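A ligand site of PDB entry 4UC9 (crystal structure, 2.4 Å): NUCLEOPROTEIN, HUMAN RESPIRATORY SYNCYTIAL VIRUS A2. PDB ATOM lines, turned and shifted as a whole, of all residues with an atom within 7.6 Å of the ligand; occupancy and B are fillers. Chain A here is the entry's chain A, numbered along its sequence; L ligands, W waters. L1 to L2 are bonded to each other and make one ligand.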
ATOM      1  N   LYS A  19     -15.292  -4.946 -19.948  1.00  0.00           N
ATOM      2  CA  LYS A  19     -14.439  -6.117 -19.698  1.00  0.00           C
ATOM      3  C   LYS A  19     -13.315  -5.806 -18.693  1.00  0.00           C
ATOM      4  O   LYS A  19     -12.971  -6.676 -17.891  1.00  0.00           O
ATOM      5  CB  LYS A  19     -13.874  -6.677 -21.034  1.00  0.00           C
ATOM      6  CG  LYS A  19     -13.166  -8.018 -20.909  1.00  0.00           C
ATOM      7  CD  LYS A  19     -12.827  -8.602 -22.252  1.00  0.00           C
ATOM      8  CE  LYS A  19     -11.796  -9.703 -22.131  1.00  0.00           C
ATOM      9  NZ  LYS A  19     -12.276 -10.981 -22.717  1.00  0.00           N
ATOM     10  N   GLY A  22     -14.960  -5.867 -15.201  1.00  0.00           N
ATOM     11  CA  GLY A  22     -15.162  -7.286 -14.912  1.00  0.00           C
ATOM     12  C   GLY A  22     -13.868  -8.027 -14.644  1.00  0.00           C
ATOM     13  O   GLY A  22     -13.881  -8.997 -13.883  1.00  0.00           O
ATOM     14  N   MET A  23     -12.731  -7.570 -15.240  1.00  0.00           N
ATOM     15  CA  MET A  23     -11.454  -8.205 -14.940  1.00  0.00           C
ATOM     16  C   MET A  23     -11.123  -7.974 -13.480  1.00  0.00           C
ATOM     17  O   MET A  23     -10.802  -8.932 -12.769  1.00  0.00           O
ATOM     18  CB  MET A  23     -10.337  -7.777 -15.889  1.00  0.00           C
ATOM     19  CG  MET A  23     -10.487  -8.389 -17.256  1.00  0.00           C
ATOM     20  SD  MET A  23      -9.105  -8.130 -18.391  1.00  0.00           S
ATOM     21  CE  MET A  23      -9.098  -6.386 -18.560  1.00  0.00           C
ATOM     22  N   ILE A  26     -13.406 -10.092 -11.073  1.00  0.00           N
ATOM     23  CA  ILE A  26     -13.077 -11.518 -10.906  1.00  0.00           C
ATOM     24  C   ILE A  26     -11.802 -11.714 -10.067  1.00  0.00           C
ATOM     25  O   ILE A  26     -11.594 -12.822  -9.584  1.00  0.00           O
ATOM     26  CB  ILE A  26     -13.053 -12.386 -12.216  1.00  0.00           C
ATOM     27  CG1 ILE A  26     -11.852 -12.034 -13.133  1.00  0.00           C
ATOM     28  CG2 ILE A  26     -14.395 -12.306 -12.936  1.00  0.00           C
ATOM     29  CD1 ILE A  26     -11.494 -13.108 -14.384  1.00  0.00           C
ATOM     30  N   MET A  82       2.852 -12.792 -25.294  1.00  0.00           N
ATOM     31  CA  MET A  82       1.430 -12.578 -25.105  1.00  0.00           C
ATOM     32  C   MET A  82       0.954 -11.300 -25.785  1.00  0.00           C
ATOM     33  O   MET A  82       1.665 -10.295 -25.772  1.00  0.00           O
ATOM     34  CB  MET A  82       1.093 -12.537 -23.603  1.00  0.00           C
ATOM     35  CG  MET A  82       0.877 -13.907 -22.959  1.00  0.00           C
ATOM     36  SD  MET A  82      -0.868 -14.424 -22.826  1.00  0.00           S
ATOM     37  CE  MET A  82      -1.431 -13.483 -21.427  1.00  0.00           C
ATOM     38  N   PHE A  84      -1.904  -8.320 -25.850  1.00  0.00           N
ATOM     39  CA  PHE A  84      -2.883  -7.636 -25.019  1.00  0.00           C
ATOM     40  C   PHE A  84      -3.536  -6.490 -25.766  1.00  0.00           C
ATOM     41  O   PHE A  84      -2.864  -5.766 -26.515  1.00  0.00           O
ATOM     42  CB  PHE A  84      -2.225  -7.089 -23.736  1.00  0.00           C
ATOM     43  CG  PHE A  84      -1.634  -8.119 -22.818  1.00  0.00           C
ATOM     44  CD1 PHE A  84      -2.414  -8.728 -21.836  1.00  0.00           C
ATOM     45  CD2 PHE A  84      -0.286  -8.479 -22.921  1.00  0.00           C
ATOM     46  CE1 PHE A  84      -1.862  -9.681 -20.979  1.00  0.00           C
ATOM     47  CE2 PHE A  84       0.260  -9.425 -22.054  1.00  0.00           C
ATOM     48  CZ  PHE A  84      -0.520 -10.032 -21.104  1.00  0.00           C
ATOM     49  N   ILE A 100      -3.597  -5.613 -14.761  1.00  0.00           N
ATOM     50  CA  ILE A 100      -5.010  -5.890 -14.425  1.00  0.00           C
ATOM     51  C   ILE A 100      -5.409  -7.224 -15.075  1.00  0.00           C
ATOM     52  O   ILE A 100      -5.875  -8.107 -14.358  1.00  0.00           O
ATOM     53  CB  ILE A 100      -5.990  -4.712 -14.738  1.00  0.00           C
ATOM     54  CG1 ILE A 100      -5.850  -3.597 -13.675  1.00  0.00           C
ATOM     55  CG2 ILE A 100      -7.448  -5.188 -14.809  1.00  0.00           C
ATOM     56  CD1 ILE A 100      -6.410  -2.191 -14.037  1.00  0.00           C
ATOM     57  N   GLU A 101      -5.140  -7.387 -16.404  1.00  0.00           N
ATOM     58  CA  GLU A 101      -5.428  -8.608 -17.170  1.00  0.00           C
ATOM     59  C   GLU A 101      -4.663  -9.845 -16.652  1.00  0.00           C
ATOM     60  O   GLU A 101      -5.271 -10.901 -16.517  1.00  0.00           O
ATOM     61  CB  GLU A 101      -5.192  -8.411 -18.685  1.00  0.00           C
ATOM     62  CG  GLU A 101      -5.845  -9.474 -19.568  1.00  0.00           C
ATOM     63  CD  GLU A 101      -5.778  -9.304 -21.068  1.00  0.00           C
ATOM     64  OE1 GLU A 101      -5.958  -8.168 -21.562  1.00  0.00           O
ATOM     65  OE2 GLU A 101      -5.591 -10.330 -21.772  1.00  0.00           O
ATOM     66  N   ILE A 102      -3.365  -9.685 -16.320  1.00  0.00           N
ATOM     67  CA  ILE A 102      -2.512 -10.758 -15.800  1.00  0.00           C
ATOM     68  C   ILE A 102      -3.039 -11.284 -14.465  1.00  0.00           C
ATOM     69  O   ILE A 102      -3.168 -12.499 -14.305  1.00  0.00           O
ATOM     70  CB  ILE A 102      -0.999 -10.343 -15.746  1.00  0.00           C
ATOM     71  CG1 ILE A 102      -0.433 -10.169 -17.168  1.00  0.00           C
ATOM     72  CG2 ILE A 102      -0.155 -11.354 -14.938  1.00  0.00           C
ATOM     73  CD1 ILE A 102       0.840  -9.353 -17.253  1.00  0.00           C
ATOM     74  N   GLU A 103      -3.402 -10.386 -13.548  1.00  0.00           N
ATOM     75  CA  GLU A 103      -3.982 -10.748 -12.249  1.00  0.00           C
ATOM     76  C   GLU A 103      -5.343 -11.463 -12.389  1.00  0.00           C
ATOM     77  O   GLU A 103      -5.559 -12.453 -11.692  1.00  0.00           O
ATOM     78  CB  GLU A 103      -4.092  -9.515 -11.323  1.00  0.00           C
ATOM     79  CG  GLU A 103      -2.774  -9.072 -10.713  1.00  0.00           C
ATOM     80  CD  GLU A 103      -2.020 -10.152  -9.947  1.00  0.00           C
ATOM     81  OE1 GLU A 103      -2.477 -10.528  -8.842  1.00  0.00           O
ATOM     82  OE2 GLU A 103      -1.006 -10.664 -10.478  1.00  0.00           O
ATOM     83  N   SER A 104      -6.229 -10.992 -13.302  1.00  0.00           N
ATOM     84  CA  SER A 104      -7.568 -11.589 -13.523  1.00  0.00           C
ATOM     85  C   SER A 104      -7.500 -12.963 -14.214  1.00  0.00           C
ATOM     86  O   SER A 104      -8.314 -13.832 -13.886  1.00  0.00           O
ATOM     87  CB  SER A 104      -8.514 -10.635 -14.250  1.00  0.00           C
ATOM     88  OG  SER A 104      -8.097 -10.365 -15.573  1.00  0.00           O
ATOM     89  N   ARG A 105      -6.532 -13.162 -15.137  1.00  0.00           N
ATOM     90  CA  ARG A 105      -6.300 -14.462 -15.779  1.00  0.00           C
ATOM     91  C   ARG A 105      -5.893 -15.532 -14.727  1.00  0.00           C
ATOM     92  O   ARG A 105      -6.260 -16.694 -14.890  1.00  0.00           O
ATOM     93  CB  ARG A 105      -5.238 -14.379 -16.893  1.00  0.00           C
ATOM     94  CG  ARG A 105      -5.786 -13.790 -18.201  1.00  0.00           C
ATOM     95  CD  ARG A 105      -4.719 -13.570 -19.253  1.00  0.00           C
ATOM     96  NE  ARG A 105      -5.295 -13.368 -20.577  1.00  0.00           N
ATOM     97  CZ  ARG A 105      -5.469 -14.338 -21.479  1.00  0.00           C
ATOM     98  NH1 ARG A 105      -5.093 -15.580 -21.214  1.00  0.00           N
ATOM     99  NH2 ARG A 105      -6.023 -14.055 -22.658  1.00  0.00           N
ATOM    100  N   LYS A 106      -5.183 -15.116 -13.642  1.00  0.00           N
ATOM    101  CA  LYS A 106      -4.776 -15.999 -12.536  1.00  0.00           C
ATOM    102  C   LYS A 106      -5.994 -16.467 -11.748  1.00  0.00           C
ATOM    103  O   LYS A 106      -6.106 -17.647 -11.412  1.00  0.00           O
ATOM    104  CB  LYS A 106      -3.767 -15.316 -11.603  1.00  0.00           C
ATOM    105  CG  LYS A 106      -2.344 -15.297 -12.123  1.00  0.00           C
ATOM    106  CD  LYS A 106      -1.447 -14.490 -11.206  1.00  0.00           C
ATOM    107  CE  LYS A 106      -0.245 -13.957 -11.934  1.00  0.00           C
ATOM    108  NZ  LYS A 106       0.767 -13.364 -11.012  1.00  0.00           N
ATOM    109  N   SER A 107      -6.908 -15.529 -11.439  1.00  0.00           N
ATOM    110  CA  SER A 107      -8.148 -15.837 -10.723  1.00  0.00           C
ATOM    111  C   SER A 107      -9.100 -16.660 -11.605  1.00  0.00           C
ATOM    112  O   SER A 107      -9.728 -17.582 -11.091  1.00  0.00           O
ATOM    113  CB  SER A 107      -8.805 -14.568 -10.219  1.00  0.00           C
ATOM    114  OG  SER A 107      -7.994 -13.963  -9.224  1.00  0.00           O
ATOM    115  N   TYR A 108      -9.150 -16.365 -12.936  1.00  0.00           N
ATOM    116  CA  TYR A 108      -9.948 -17.125 -13.900  1.00  0.00           C
ATOM    117  C   TYR A 108      -9.487 -18.589 -13.945  1.00  0.00           C
ATOM    118  O   TYR A 108     -10.342 -19.483 -13.957  1.00  0.00           O
ATOM    119  CB  TYR A 108      -9.909 -16.508 -15.306  1.00  0.00           C
ATOM    120  CG  TYR A 108     -10.823 -17.206 -16.294  1.00  0.00           C
ATOM    121  CD1 TYR A 108     -12.163 -16.877 -16.383  1.00  0.00           C
ATOM    122  CD2 TYR A 108     -10.329 -18.200 -17.151  1.00  0.00           C
ATOM    123  CE1 TYR A 108     -13.018 -17.542 -17.274  1.00  0.00           C
ATOM    124  CE2 TYR A 108     -11.176 -18.871 -18.043  1.00  0.00           C
ATOM    125  CZ  TYR A 108     -12.519 -18.550 -18.087  1.00  0.00           C
ATOM    126  OH  TYR A 108     -13.365 -19.220 -18.938  1.00  0.00           O
ATOM    127  N   LYS A 109      -8.152 -18.824 -13.948  1.00  0.00           N
ATOM    128  CA  LYS A 109      -7.537 -20.155 -13.965  1.00  0.00           C
ATOM    129  C   LYS A 109      -7.967 -20.919 -12.699  1.00  0.00           C
ATOM    130  O   LYS A 109      -8.345 -22.082 -12.808  1.00  0.00           O
ATOM    131  CB  LYS A 109      -6.014 -20.040 -14.035  1.00  0.00           C
ATOM    132  CG  LYS A 109      -5.278 -21.301 -14.440  1.00  0.00           C
ATOM    133  CD  LYS A 109      -3.759 -21.130 -14.304  1.00  0.00           C
ATOM    134  CE  LYS A 109      -2.956 -22.341 -14.690  1.00  0.00           C
ATOM    135  NZ  LYS A 109      -1.498 -22.122 -14.481  1.00  0.00           N
ATOM    136  N   LEU A 112     -11.747 -21.994 -12.914  1.00  0.00           N
ATOM    137  CA  LEU A 112     -11.826 -23.114 -13.841  1.00  0.00           C
ATOM    138  C   LEU A 112     -11.485 -24.440 -13.148  1.00  0.00           C
ATOM    139  O   LEU A 112     -12.112 -25.461 -13.432  1.00  0.00           O
ATOM    140  CB  LEU A 112     -10.859 -22.858 -15.008  1.00  0.00           C
ATOM    141  CG  LEU A 112     -11.341 -23.050 -16.439  1.00  0.00           C
ATOM    142  CD1 LEU A 112     -12.668 -22.326 -16.708  1.00  0.00           C
ATOM    143  CD2 LEU A 112     -10.296 -22.509 -17.400  1.00  0.00           C
ATOM    144  N   GLU A 117     -16.368 -25.119 -15.560  1.00  0.00           N
ATOM    145  CA  GLU A 117     -16.756 -24.244 -16.657  1.00  0.00           C
ATOM    146  C   GLU A 117     -17.366 -23.003 -16.041  1.00  0.00           C
ATOM    147  O   GLU A 117     -18.243 -23.131 -15.177  1.00  0.00           O
ATOM    148  CB  GLU A 117     -17.759 -24.957 -17.596  1.00  0.00           C
ATOM    149  CG  GLU A 117     -18.128 -24.137 -18.829  1.00  0.00           C
ATOM    150  CD  GLU A 117     -19.169 -24.758 -19.740  1.00  0.00           C
ATOM    151  OE1 GLU A 117     -18.824 -25.717 -20.464  1.00  0.00           O
ATOM    152  OE2 GLU A 117     -20.313 -24.248 -19.766  1.00  0.00           O
ATOM    153  N   VAL A 118     -16.884 -21.809 -16.433  1.00  0.00           N
ATOM    154  CA  VAL A 118     -17.408 -20.560 -15.855  1.00  0.00           C
ATOM    155  C   VAL A 118     -18.713 -20.136 -16.530  1.00  0.00           C
ATOM    156  O   VAL A 118     -18.730 -19.892 -17.731  1.00  0.00           O
ATOM    157  CB  VAL A 118     -16.376 -19.398 -15.806  1.00  0.00           C
ATOM    158  CG1 VAL A 118     -16.925 -18.202 -15.025  1.00  0.00           C
ATOM    159  CG2 VAL A 118     -15.043 -19.867 -15.220  1.00  0.00           C
ATOM    160  N   ARG A 123     -18.424 -14.580 -15.329  1.00  0.00           N
ATOM    161  CA  ARG A 123     -17.354 -14.173 -16.244  1.00  0.00           C
ATOM    162  C   ARG A 123     -17.006 -12.674 -16.161  1.00  0.00           C
ATOM    163  O   ARG A 123     -17.832 -11.847 -15.771  1.00  0.00           O
ATOM    164  CB  ARG A 123     -17.701 -14.547 -17.691  1.00  0.00           C
ATOM    165  CG  ARG A 123     -17.598 -16.041 -18.009  1.00  0.00           C
ATOM    166  CD  ARG A 123     -17.971 -16.380 -19.470  1.00  0.00           C
ATOM    167  NE  ARG A 123     -17.077 -15.721 -20.420  1.00  0.00           N
ATOM    168  CZ  ARG A 123     -15.866 -16.156 -20.753  1.00  0.00           C
ATOM    169  NH1 ARG A 123     -15.404 -17.291 -20.256  1.00  0.00           N
ATOM    170  NH2 ARG A 123     -15.111 -15.463 -21.593  1.00  0.00           N
ATOM    171  N   HIS A 124     -15.771 -12.337 -16.571  1.00  0.00           N
ATOM    172  CA  HIS A 124     -15.238 -10.987 -16.643  1.00  0.00           C
ATOM    173  C   HIS A 124     -15.882 -10.181 -17.795  1.00  0.00           C
ATOM    174  O   HIS A 124     -15.818  -8.951 -17.760  1.00  0.00           O
ATOM    175  CB  HIS A 124     -13.737 -11.031 -16.872  1.00  0.00           C
ATOM    176  CG  HIS A 124     -13.314 -12.012 -17.937  1.00  0.00           C
ATOM    177  ND1 HIS A 124     -13.329 -13.372 -17.714  1.00  0.00           N
ATOM    178  CD2 HIS A 124     -12.843 -11.776 -19.190  1.00  0.00           C
ATOM    179  CE1 HIS A 124     -12.886 -13.934 -18.832  1.00  0.00           C
ATOM    180  NE2 HIS A 124     -12.583 -13.017 -19.746  1.00  0.00           N
ATOM    181  N   ASP A 125     -16.459 -10.862 -18.814  1.00  0.00           N
ATOM    182  CA  ASP A 125     -17.061 -10.161 -19.950  1.00  0.00           C
ATOM    183  C   ASP A 125     -18.596 -10.141 -19.897  1.00  0.00           C
ATOM    184  O   ASP A 125     -19.242  -9.863 -20.924  1.00  0.00           O
ATOM    185  CB  ASP A 125     -16.515 -10.694 -21.310  1.00  0.00           C
ATOM    186  CG  ASP A 125     -16.718 -12.169 -21.652  1.00  0.00           C
ATOM    187  OD1 ASP A 125     -17.238 -12.920 -20.778  1.00  0.00           O
ATOM    188  OD2 ASP A 125     -16.386 -12.565 -22.796  1.00  0.00           O
HETATM  189  N1  LIG L   1     -10.109 -20.080 -21.753  1.00  0.00           N
HETATM  190  C1  LIG L   1     -11.367 -19.513 -22.270  1.00  0.00           C
HETATM  191  C2  LIG L   1     -11.564 -18.023 -21.914  1.00  0.00           C
HETATM  192  O1  LIG L   1     -12.680 -17.501 -21.999  1.00  0.00           O
HETATM  193  C3  LIG L   1     -12.570 -20.355 -21.829  1.00  0.00           C
HETATM  194  N1  LG2 L   2     -10.457 -17.334 -21.538  1.00  0.00           N
HETATM  195  C1  LG2 L   2     -10.395 -15.920 -21.158  1.00  0.00           C
HETATM  196  C2  LG2 L   2     -10.742 -14.953 -22.344  1.00  0.00           C
HETATM  197  O1  LG2 L   2     -10.238 -15.166 -23.464  1.00  0.00           O
HETATM  198  C3  LG2 L   2      -9.018 -15.592 -20.533  1.00  0.00           C
HETATM  199  C4  LG2 L   2      -8.995 -14.286 -19.771  1.00  0.00           C
HETATM  200  C5  LG2 L   2      -9.402 -14.232 -18.436  1.00  0.00           C
HETATM  201  C6  LG2 L   2      -8.613 -13.105 -20.392  1.00  0.00           C
HETATM  202  C7  LG2 L   2      -9.403 -13.018 -17.743  1.00  0.00           C
HETATM  203  C8  LG2 L   2      -8.623 -11.886 -19.698  1.00  0.00           C
HETATM  204  C9  LG2 L   2      -9.010 -11.859 -18.372  1.00  0.00           C
HETATM  205  O2  LG2 L   2     -11.503 -13.969 -22.134  1.00  0.00           O
HETATM  206  O   HOH W   1     -13.895 -13.416 -23.199  1.00  0.00           O
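The guanidinium group (NH2) of Arg 123 lies within salt-bridge range of an oxygen (O2) of LG2 L2 (3.9 Å).
A ring nitrogen (NE2) of His 124 sits at hydrogen-bond distance from an oxygen (O2) of LG2 L2.
An oxygen (O2) of LG2 L2 lies within salt-bridge range of the side-chain amino group (NZ) of Lys 19 (3.1 Å).
The side-chain hydroxyl (OG) of Ser 104 sits at hydrogen-bond distance from the backbone carbonyl oxygen (O) of Glu 101 (3.0 Å).
NE of Arg 123 is in salt-bridge range of OD1 of Asp 125 (2.8 Å).
The side-chain hydroxyl of Tyr 108 lies within hydrogen-bond range of the guanidinium group of Arg 123 (3.1 Å).
The side-chain sulfur (SD) of Met 23 lies close to the side-chain hydroxyl (OG) of Ser 104, at 3.7 Å.
NE of Arg 105 lies within salt-bridge range of OE2 of Glu 101 (3.3 Å).
OG of Ser 104 lies within hydrogen-bond range of O of Ile 100, at 3.4 Å.
Residues that only touch the ligand: Met 23 (3.7 Å), Ile 26 (3.96 Å), Glu 101 (3.7 Å), Ser 104 (3.3 Å), Arg 105 (3.3 Å) and Tyr 108 (3.2 Å).
Hydrophobic or aromatic side chains that line the ligand: Met 23, Ile 26, Tyr 108 and His 124.
Along chain A the residues within 4 Å of the ligand span positions 19 to 124.
Water W1 lies within hydrogen-bond range of the side-chain carboxylate of Asp 125, an oxygen (O2) of LG2 L2, the guanidinium group of Arg 123 and the side-chain amino group of Lys 19.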
